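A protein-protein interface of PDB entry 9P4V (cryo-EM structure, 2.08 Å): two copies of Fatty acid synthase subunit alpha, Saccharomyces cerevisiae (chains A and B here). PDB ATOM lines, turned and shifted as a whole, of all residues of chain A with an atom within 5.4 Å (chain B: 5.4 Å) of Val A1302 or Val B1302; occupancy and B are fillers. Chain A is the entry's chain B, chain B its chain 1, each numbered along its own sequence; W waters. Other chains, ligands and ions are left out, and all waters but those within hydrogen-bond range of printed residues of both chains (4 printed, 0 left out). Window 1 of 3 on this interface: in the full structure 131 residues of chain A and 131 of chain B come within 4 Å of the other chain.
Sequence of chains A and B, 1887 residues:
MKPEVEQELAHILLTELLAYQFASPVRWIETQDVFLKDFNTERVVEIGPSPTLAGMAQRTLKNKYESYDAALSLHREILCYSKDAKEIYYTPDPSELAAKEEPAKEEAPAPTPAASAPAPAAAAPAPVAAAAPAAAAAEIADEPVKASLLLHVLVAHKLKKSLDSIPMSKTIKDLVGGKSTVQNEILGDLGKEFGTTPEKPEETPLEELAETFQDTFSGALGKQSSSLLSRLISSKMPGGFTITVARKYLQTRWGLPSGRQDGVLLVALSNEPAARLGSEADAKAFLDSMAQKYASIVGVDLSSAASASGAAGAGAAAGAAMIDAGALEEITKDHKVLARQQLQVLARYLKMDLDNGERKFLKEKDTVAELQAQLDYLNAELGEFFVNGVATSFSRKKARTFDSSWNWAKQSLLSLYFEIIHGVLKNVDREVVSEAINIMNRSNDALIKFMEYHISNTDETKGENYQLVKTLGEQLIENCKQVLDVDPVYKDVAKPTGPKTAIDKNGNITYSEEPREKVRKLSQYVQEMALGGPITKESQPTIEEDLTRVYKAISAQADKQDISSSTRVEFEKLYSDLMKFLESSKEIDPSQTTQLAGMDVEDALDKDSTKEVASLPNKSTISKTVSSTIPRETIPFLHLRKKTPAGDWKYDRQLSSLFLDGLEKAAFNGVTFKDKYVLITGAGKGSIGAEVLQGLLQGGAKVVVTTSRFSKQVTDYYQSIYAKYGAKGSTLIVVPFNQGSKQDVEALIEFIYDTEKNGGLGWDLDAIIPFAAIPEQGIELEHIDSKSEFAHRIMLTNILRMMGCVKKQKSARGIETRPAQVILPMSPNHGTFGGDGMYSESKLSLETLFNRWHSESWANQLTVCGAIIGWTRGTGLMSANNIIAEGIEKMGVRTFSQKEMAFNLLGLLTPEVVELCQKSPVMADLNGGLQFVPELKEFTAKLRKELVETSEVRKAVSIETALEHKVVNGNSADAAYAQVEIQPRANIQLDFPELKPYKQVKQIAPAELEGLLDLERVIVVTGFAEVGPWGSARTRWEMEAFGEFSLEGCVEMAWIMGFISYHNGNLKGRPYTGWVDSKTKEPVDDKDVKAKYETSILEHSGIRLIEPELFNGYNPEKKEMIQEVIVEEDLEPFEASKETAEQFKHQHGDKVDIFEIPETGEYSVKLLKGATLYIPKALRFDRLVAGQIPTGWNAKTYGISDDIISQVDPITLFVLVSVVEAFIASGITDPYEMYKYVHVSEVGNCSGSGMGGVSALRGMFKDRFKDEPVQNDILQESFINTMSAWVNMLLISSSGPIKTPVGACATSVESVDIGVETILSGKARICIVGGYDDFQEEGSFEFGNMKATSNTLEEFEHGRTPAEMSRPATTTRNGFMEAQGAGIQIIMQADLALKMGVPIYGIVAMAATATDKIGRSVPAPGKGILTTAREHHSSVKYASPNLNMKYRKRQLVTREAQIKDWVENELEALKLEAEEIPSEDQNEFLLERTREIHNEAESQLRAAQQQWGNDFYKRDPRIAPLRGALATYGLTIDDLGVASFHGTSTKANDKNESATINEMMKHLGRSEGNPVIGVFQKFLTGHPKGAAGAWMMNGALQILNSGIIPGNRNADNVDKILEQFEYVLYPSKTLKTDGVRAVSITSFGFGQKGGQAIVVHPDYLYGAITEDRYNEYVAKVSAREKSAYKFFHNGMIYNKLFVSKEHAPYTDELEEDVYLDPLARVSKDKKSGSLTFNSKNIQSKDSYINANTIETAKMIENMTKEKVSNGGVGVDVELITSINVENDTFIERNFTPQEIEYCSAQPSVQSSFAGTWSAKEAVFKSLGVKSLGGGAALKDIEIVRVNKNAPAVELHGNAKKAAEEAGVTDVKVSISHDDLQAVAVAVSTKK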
ATOM      1  N   SER A1249       6.140   5.824 -12.766  1.00  0.00           N
ATOM      2  CA  SER A1249       5.194   4.939 -12.116  1.00  0.00           C
ATOM      3  C   SER A1249       5.845   4.308 -10.897  1.00  0.00           C
ATOM      4  O   SER A1249       7.060   4.121 -10.856  1.00  0.00           O
ATOM      5  CB  SER A1249       4.721   3.845 -13.068  1.00  0.00           C
ATOM      6  OG  SER A1249       3.744   3.038 -12.459  1.00  0.00           O
ATOM      7  N   GLY A1250       5.019   3.980  -9.907  1.00  0.00           N
ATOM      8  CA  GLY A1250       5.513   3.240  -8.762  1.00  0.00           C
ATOM      9  C   GLY A1250       5.804   1.789  -9.091  1.00  0.00           C
ATOM     10  O   GLY A1250       6.808   1.235  -8.646  1.00  0.00           O
ATOM     11  N   MET A1251       4.945   1.164  -9.893  1.00  0.00           N
ATOM     12  CA  MET A1251       5.024  -0.270 -10.135  1.00  0.00           C
ATOM     13  C   MET A1251       4.857  -0.678 -11.591  1.00  0.00           C
ATOM     14  O   MET A1251       5.150  -1.828 -11.912  1.00  0.00           O
ATOM     15  CB  MET A1251       3.965  -0.992  -9.290  1.00  0.00           C
ATOM     16  CG  MET A1251       4.419  -1.336  -7.888  1.00  0.00           C
ATOM     17  SD  MET A1251       5.774  -2.539  -7.815  1.00  0.00           S
ATOM     18  CE  MET A1251       5.170  -3.838  -8.893  1.00  0.00           C
ATOM     19  N   ILE A1280       8.154  -0.241 -16.211  1.00  0.00           N
ATOM     20  CA  ILE A1280       7.632   1.056 -15.824  1.00  0.00           C
ATOM     21  C   ILE A1280       7.801   2.063 -16.956  1.00  0.00           C
ATOM     22  O   ILE A1280       6.963   2.935 -17.116  1.00  0.00           O
ATOM     23  CB  ILE A1280       8.273   1.554 -14.514  1.00  0.00           C
ATOM     24  CG1 ILE A1280       7.625   0.822 -13.337  1.00  0.00           C
ATOM     25  CG2 ILE A1280       8.113   3.058 -14.363  1.00  0.00           C
ATOM     26  CD1 ILE A1280       8.256   1.091 -11.989  1.00  0.00           C
ATOM     27  N   ASN A1281       8.845   1.909 -17.765  1.00  0.00           N
ATOM     28  CA  ASN A1281       9.087   2.847 -18.863  1.00  0.00           C
ATOM     29  C   ASN A1281       8.395   2.489 -20.186  1.00  0.00           C
ATOM     30  O   ASN A1281       8.476   3.247 -21.143  1.00  0.00           O
ATOM     31  CB  ASN A1281      10.584   3.003 -19.115  1.00  0.00           C
ATOM     32  CG  ASN A1281      11.226   1.725 -19.613  1.00  0.00           C
ATOM     33  OD1 ASN A1281      11.271   0.726 -18.905  1.00  0.00           O
ATOM     34  ND2 ASN A1281      11.730   1.754 -20.834  1.00  0.00           N
ATOM     35  N   THR A1300      12.451   8.134 -16.850  1.00  0.00           N
ATOM     36  CA  THR A1300      11.289   7.614 -16.138  1.00  0.00           C
ATOM     37  C   THR A1300      11.586   7.415 -14.648  1.00  0.00           C
ATOM     38  O   THR A1300      12.322   6.512 -14.286  1.00  0.00           O
ATOM     39  CB  THR A1300      10.813   6.279 -16.752  1.00  0.00           C
ATOM     40  OG1 THR A1300      10.720   6.409 -18.174  1.00  0.00           O
ATOM     41  CG2 THR A1300       9.461   5.872 -16.184  1.00  0.00           C
ATOM     42  N   PRO A1301      11.014   8.260 -13.783  1.00  0.00           N
ATOM     43  CA  PRO A1301      11.230   8.083 -12.343  1.00  0.00           C
ATOM     44  C   PRO A1301      10.396   6.947 -11.772  1.00  0.00           C
ATOM     45  O   PRO A1301       9.384   6.533 -12.328  1.00  0.00           O
ATOM     46  CB  PRO A1301      10.796   9.422 -11.740  1.00  0.00           C
ATOM     47  CG  PRO A1301       9.972  10.091 -12.769  1.00  0.00           C
ATOM     48  CD  PRO A1301      10.105   9.378 -14.076  1.00  0.00           C
ATOM     49  N   VAL A1302      10.861   6.434 -10.641  1.00  0.00           N
ATOM     50  CA  VAL A1302      10.113   5.495  -9.817  1.00  0.00           C
ATOM     51  C   VAL A1302      10.240   6.000  -8.389  1.00  0.00           C
ATOM     52  O   VAL A1302      11.326   5.949  -7.805  1.00  0.00           O
ATOM     53  CB  VAL A1302      10.620   4.051  -9.949  1.00  0.00           C
ATOM     54  CG1 VAL A1302       9.860   3.119  -9.016  1.00  0.00           C
ATOM     55  CG2 VAL A1302      10.481   3.576 -11.368  1.00  0.00           C
ATOM     56  N   GLY A1303       9.149   6.512  -7.838  1.00  0.00           N
ATOM     57  CA  GLY A1303       9.204   7.148  -6.541  1.00  0.00           C
ATOM     58  C   GLY A1303       8.070   6.752  -5.628  1.00  0.00           C
ATOM     59  O   GLY A1303       7.638   7.555  -4.803  1.00  0.00           O
ATOM     60  N   ALA A1304       7.599   5.514  -5.754  1.00  0.00           N
ATOM     61  CA  ALA A1304       6.438   5.034  -5.015  1.00  0.00           C
ATOM     62  C   ALA A1304       5.310   6.064  -5.066  1.00  0.00           C
ATOM     63  O   ALA A1304       4.807   6.374  -6.147  1.00  0.00           O
ATOM     64  CB  ALA A1304       6.821   4.692  -3.573  1.00  0.00           C
ATOM     65  N   THR A1307       5.966   9.712  -6.930  1.00  0.00           N
ATOM     66  CA  THR A1307       6.461   9.614  -8.299  1.00  0.00           C
ATOM     67  C   THR A1307       6.147  10.870  -9.100  1.00  0.00           C
ATOM     68  O   THR A1307       6.998  11.367  -9.834  1.00  0.00           O
ATOM     69  CB  THR A1307       5.853   8.392  -8.988  1.00  0.00           C
ATOM     70  OG1 THR A1307       6.385   7.197  -8.415  1.00  0.00           O
ATOM     71  CG2 THR A1307       6.159   8.405 -10.475  1.00  0.00           C
ATOM     72  N   GLU A1310       8.416  13.779  -8.110  1.00  0.00           N
ATOM     73  CA  GLU A1310       9.739  13.507  -8.667  1.00  0.00           C
ATOM     74  C   GLU A1310       9.756  13.765 -10.171  1.00  0.00           C
ATOM     75  O   GLU A1310      10.717  14.325 -10.710  1.00  0.00           O
ATOM     76  CB  GLU A1310      10.135  12.065  -8.355  1.00  0.00           C
ATOM     77  CG  GLU A1310      11.369  11.558  -9.065  1.00  0.00           C
ATOM     78  CD  GLU A1310      11.811  10.195  -8.556  1.00  0.00           C
ATOM     79  OE1 GLU A1310      11.420   9.820  -7.436  1.00  0.00           O
ATOM     80  OE2 GLU A1310      12.541   9.490  -9.277  1.00  0.00           O
ATOM     81  N   LYS A1649      10.884   8.767   0.105  1.00  0.00           N
ATOM     82  CA  LYS A1649      10.714   9.650  -1.046  1.00  0.00           C
ATOM     83  C   LYS A1649       9.853  10.835  -0.623  1.00  0.00           C
ATOM     84  O   LYS A1649       8.626  10.758  -0.628  1.00  0.00           O
ATOM     85  CB  LYS A1649      10.096   8.895  -2.215  1.00  0.00           C
ATOM     86  CG  LYS A1649      11.058   7.990  -2.949  1.00  0.00           C
ATOM     87  CD  LYS A1649      11.524   8.591  -4.259  1.00  0.00           C
ATOM     88  CE  LYS A1649      12.474   7.651  -4.991  1.00  0.00           C
ATOM     89  NZ  LYS A1649      12.767   8.071  -6.383  1.00  0.00           N
ATOM     90  N   SER B1249      17.240   0.971 -11.590  1.00  0.00           N
ATOM     91  CA  SER B1249      17.147  -0.436 -11.920  1.00  0.00           C
ATOM     92  C   SER B1249      16.121  -0.631 -13.023  1.00  0.00           C
ATOM     93  O   SER B1249      15.171   0.140 -13.146  1.00  0.00           O
ATOM     94  CB  SER B1249      16.750  -1.262 -10.700  1.00  0.00           C
ATOM     95  OG  SER B1249      16.740  -2.635 -11.005  1.00  0.00           O
ATOM     96  N   GLY B1250      16.326  -1.676 -13.823  1.00  0.00           N
ATOM     97  CA  GLY B1250      15.332  -2.039 -14.813  1.00  0.00           C
ATOM     98  C   GLY B1250      14.099  -2.668 -14.195  1.00  0.00           C
ATOM     99  O   GLY B1250      12.975  -2.376 -14.602  1.00  0.00           O
ATOM    100  N   MET B1251      14.289  -3.516 -13.186  1.00  0.00           N
ATOM    101  CA  MET B1251      13.201  -4.310 -12.635  1.00  0.00           C
ATOM    102  C   MET B1251      13.160  -4.361 -11.115  1.00  0.00           C
ATOM    103  O   MET B1251      12.147  -4.799 -10.572  1.00  0.00           O
ATOM    104  CB  MET B1251      13.283  -5.743 -13.179  1.00  0.00           C
ATOM    105  CG  MET B1251      12.581  -5.944 -14.505  1.00  0.00           C
ATOM    106  SD  MET B1251      10.783  -5.719 -14.441  1.00  0.00           S
ATOM    107  CE  MET B1251      10.335  -6.744 -13.039  1.00  0.00           C
ATOM    108  N   ILE B1280      11.769  -0.592  -7.081  1.00  0.00           N
ATOM    109  CA  ILE B1280      13.036  -0.245  -7.697  1.00  0.00           C
ATOM    110  C   ILE B1280      13.786   0.775  -6.848  1.00  0.00           C
ATOM    111  O   ILE B1280      15.005   0.743  -6.805  1.00  0.00           O
ATOM    112  CB  ILE B1280      12.844   0.245  -9.145  1.00  0.00           C
ATOM    113  CG1 ILE B1280      12.611  -0.965 -10.052  1.00  0.00           C
ATOM    114  CG2 ILE B1280      14.047   1.045  -9.617  1.00  0.00           C
ATOM    115  CD1 ILE B1280      12.251  -0.635 -11.482  1.00  0.00           C
ATOM    116  N   ASN B1281      13.061   1.633  -6.137  1.00  0.00           N
ATOM    117  CA  ASN B1281      13.709   2.657  -5.312  1.00  0.00           C
ATOM    118  C   ASN B1281      14.040   2.219  -3.878  1.00  0.00           C
ATOM    119  O   ASN B1281      14.647   2.977  -3.133  1.00  0.00           O
ATOM    120  CB  ASN B1281      12.855   3.920  -5.258  1.00  0.00           C
ATOM    121  CG  ASN B1281      11.533   3.700  -4.551  1.00  0.00           C
ATOM    122  OD1 ASN B1281      10.692   2.941  -5.014  1.00  0.00           O
ATOM    123  ND2 ASN B1281      11.347   4.370  -3.427  1.00  0.00           N
ATOM    124  N   THR B1300      15.177   8.033  -8.813  1.00  0.00           N
ATOM    125  CA  THR B1300      15.491   6.683  -9.264  1.00  0.00           C
ATOM    126  C   THR B1300      14.993   6.437 -10.693  1.00  0.00           C
ATOM    127  O   THR B1300      13.798   6.329 -10.913  1.00  0.00           O
ATOM    128  CB  THR B1300      14.883   5.626  -8.317  1.00  0.00           C
ATOM    129  OG1 THR B1300      15.188   5.962  -6.959  1.00  0.00           O
ATOM    130  CG2 THR B1300      15.422   4.238  -8.634  1.00  0.00           C
ATOM    131  N   PRO B1301      15.909   6.352 -11.663  1.00  0.00           N
ATOM    132  CA  PRO B1301      15.485   6.072 -13.039  1.00  0.00           C
ATOM    133  C   PRO B1301      15.141   4.606 -13.248  1.00  0.00           C
ATOM    134  O   PRO B1301      15.564   3.721 -12.510  1.00  0.00           O
ATOM    135  CB  PRO B1301      16.703   6.460 -13.883  1.00  0.00           C
ATOM    136  CG  PRO B1301      17.851   6.508 -12.954  1.00  0.00           C
ATOM    137  CD  PRO B1301      17.371   6.454 -11.540  1.00  0.00           C
ATOM    138  N   VAL B1302      14.336   4.368 -14.274  1.00  0.00           N
ATOM    139  CA  VAL B1302      14.052   3.032 -14.780  1.00  0.00           C
ATOM    140  C   VAL B1302      14.193   3.121 -16.292  1.00  0.00           C
ATOM    141  O   VAL B1302      13.374   3.759 -16.956  1.00  0.00           O
ATOM    142  CB  VAL B1302      12.660   2.524 -14.376  1.00  0.00           C
ATOM    143  CG1 VAL B1302      12.379   1.159 -14.989  1.00  0.00           C
ATOM    144  CG2 VAL B1302      12.547   2.444 -12.879  1.00  0.00           C
ATOM    145  N   GLY B1303      15.241   2.512 -16.829  1.00  0.00           N
ATOM    146  CA  GLY B1303      15.540   2.660 -18.235  1.00  0.00           C
ATOM    147  C   GLY B1303      15.907   1.362 -18.912  1.00  0.00           C
ATOM    148  O   GLY B1303      16.703   1.362 -19.849  1.00  0.00           O
ATOM    149  N   ALA B1304      15.317   0.258 -18.459  1.00  0.00           N
ATOM    150  CA  ALA B1304      15.658  -1.073 -18.945  1.00  0.00           C
ATOM    151  C   ALA B1304      17.175  -1.244 -19.014  1.00  0.00           C
ATOM    152  O   ALA B1304      17.850  -1.174 -17.986  1.00  0.00           O
ATOM    153  CB  ALA B1304      15.001  -1.334 -20.303  1.00  0.00           C
ATOM    154  N   THR B1307      19.631   1.976 -18.109  1.00  0.00           N
ATOM    155  CA  THR B1307      19.370   2.590 -16.811  1.00  0.00           C
ATOM    156  C   THR B1307      20.591   3.335 -16.290  1.00  0.00           C
ATOM    157  O   THR B1307      20.470   4.447 -15.780  1.00  0.00           O
ATOM    158  CB  THR B1307      18.941   1.525 -15.803  1.00  0.00           C
ATOM    159  OG1 THR B1307      17.645   1.031 -16.141  1.00  0.00           O
ATOM    160  CG2 THR B1307      18.901   2.098 -14.398  1.00  0.00           C
ATOM    161  N   GLU B1310      21.133   6.630 -18.144  1.00  0.00           N
ATOM    162  CA  GLU B1310      20.111   7.563 -17.680  1.00  0.00           C
ATOM    163  C   GLU B1310      20.446   8.083 -16.284  1.00  0.00           C
ATOM    164  O   GLU B1310      20.277   9.271 -15.989  1.00  0.00           O
ATOM    165  CB  GLU B1310      18.748   6.874 -17.695  1.00  0.00           C
ATOM    166  CG  GLU B1310      17.627   7.627 -17.020  1.00  0.00           C
ATOM    167  CD  GLU B1310      16.271   6.976 -17.246  1.00  0.00           C
ATOM    168  OE1 GLU B1310      16.139   6.194 -18.206  1.00  0.00           O
ATOM    169  OE2 GLU B1310      15.339   7.234 -16.463  1.00  0.00           O
ATOM    170  N   LYS B1649      14.936   3.414 -25.212  1.00  0.00           N
ATOM    171  CA  LYS B1649      15.821   4.109 -24.281  1.00  0.00           C
ATOM    172  C   LYS B1649      17.226   4.125 -24.872  1.00  0.00           C
ATOM    173  O   LYS B1649      17.986   3.170 -24.723  1.00  0.00           O
ATOM    174  CB  LYS B1649      15.795   3.440 -22.914  1.00  0.00           C
ATOM    175  CG  LYS B1649      14.561   3.747 -22.097  1.00  0.00           C
ATOM    176  CD  LYS B1649      14.831   4.770 -21.012  1.00  0.00           C
ATOM    177  CE  LYS B1649      13.580   5.044 -20.187  1.00  0.00           C
ATOM    178  NZ  LYS B1649      13.840   5.845 -18.966  1.00  0.00           N
HETATM  179  O   HOH W   1       7.933   2.388  -6.252  1.00  0.00           O
HETATM  180  O   HOH W   2       9.174  -0.450  -8.724  1.00  0.00           O
HETATM  181  O   HOH W   3      12.799  -1.397 -17.280  1.00  0.00           O
HETATM  182  O   HOH W   4      10.186  -1.842 -14.411  1.00  0.00           O
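The side-chain hydroxyl (OG1) of Thr B1300 sits at hydrogen-bond distance from the side-chain amino group (NZ) of Lys A1649 (3.3 Å).
OG1 of Thr A1300 is in hydrogen-bond range of NZ of Lys B1649, 3.3 Å away.
N of Thr A1300 is in hydrogen-bond range of OE2 of Glu B1310, at 3.0 Å.
The backbone NH (N) of Thr B1300 is in hydrogen-bond range of the side-chain carboxylate (OE2) of Glu A1310, at 3.0 Å.
N of Val B1302 is in hydrogen-bond range of O of Thr A1300 (2.9 Å).
The backbone carbonyl oxygen (O) of Thr B1300 sits at hydrogen-bond distance from the backbone NH (N) of Val A1302 (3.0 Å).
The side-chain amino group of Lys A1649 is in hydrogen-bond range of the backbone carbonyl oxygen of Val A1302 (2.9 Å).
The side-chain carboxylate of Glu A1310 is in salt-bridge range of the side-chain amino group of Lys A1649.
N of Ser B1249 sits at hydrogen-bond distance from O of Pro B1301 (3.3 Å).
N of Ser A1249 sits at hydrogen-bond distance from O of Pro A1301 (3.3 Å).
The side-chain amino group (NZ) of Lys B1649 sits at hydrogen-bond distance from the backbone carbonyl oxygen (O) of Val B1302.
OE1 of Glu B1310 lies within salt-bridge range of NZ of Lys B1649, 2.4 Å away.
Asn A1281 touches Val B1302 (CB to O, 3.6 Å).
Lys B1649 touches Asn A1281.
Thr A1300 touches Thr B1300 (O to O, 3.7 Å).
Pro B1301 touches Thr A1300.
Pro A1301 touches Thr B1300.
CB of Asn B1281 touches O of Val A1302 (3.6 Å).
CG2 of Val B1302 touches CG2 of Val A1302 (2.8 Å).
Asn B1281 touches Lys A1649 (ND2 to CG, 3.7 Å).
Printed residues of chain B within 4 Å of Asn A1281: Val B1302 and Lys B1649.
Printed residues of chain B within 4 Å of Thr A1300: Thr B1300 (3.7 Å), Pro B1301 (3.4 Å), Val B1302 (2.9 Å), Glu B1310 (3.0 Å) and Lys B1649 (3.3 Å).
Of the printed residues of chain B, Glu A1310 touches Thr B1300.
Of the printed residues of chain A, Thr B1300 touches Thr A1300, Pro A1301, Val A1302, Glu A1310 and Lys A1649.
Of chain A, only Asn A1281, Thr A1300 and Val A1302 come within 4 Å of Val B1302.
Printed residues of chain A within 4 Å of Glu B1310: Thr A1300 (3.0 Å).
The nearest residue of chain B that does not touch Val A1302 is Ile B1280 (4.1 Å).
Of the 13 printed residues of chain B, 6 touch a printed residue of chain A.
Hydrophobic or aromatic side chains of chain B that line the printed part of chain A: Val B1302.
Hydrophobic or aromatic side chains of chain A within 4 Å of the printed part of chain B: Val A1302.
Asn A1281 touches Val B1302, and with the chains exchanged Val A1302 touches Asn B1281.
Asn A1281 touches Lys B1649, and with the chains exchanged Lys A1649 touches Asn B1281.
Thr A1300 touches Glu B1310, and with the chains exchanged Glu A1310 touches Thr B1300.
Val A1302 touches its own counterpart, Val B1302.
Water W4 bridges the backbone carbonyl oxygen of Gly B1250 (2.8 Å) and the backbone NH of Ile A1280 (3.2 Å).
Water W3 lies within hydrogen-bond range of O of Gly B1250 (2.9 Å), OD1 of Asn A1281 (3.1 Å) and N of Ala B1304 (3.2 Å).
Water W1 lies within hydrogen-bond range of O of Gly A1250 (2.9 Å), OD1 of Asn B1281 (3.1 Å) and N of Ala A1304 (3.2 Å).
Water W2 bridges O of Gly A1250 (2.9 Å) and N of Ile B1280 (3.1 Å).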
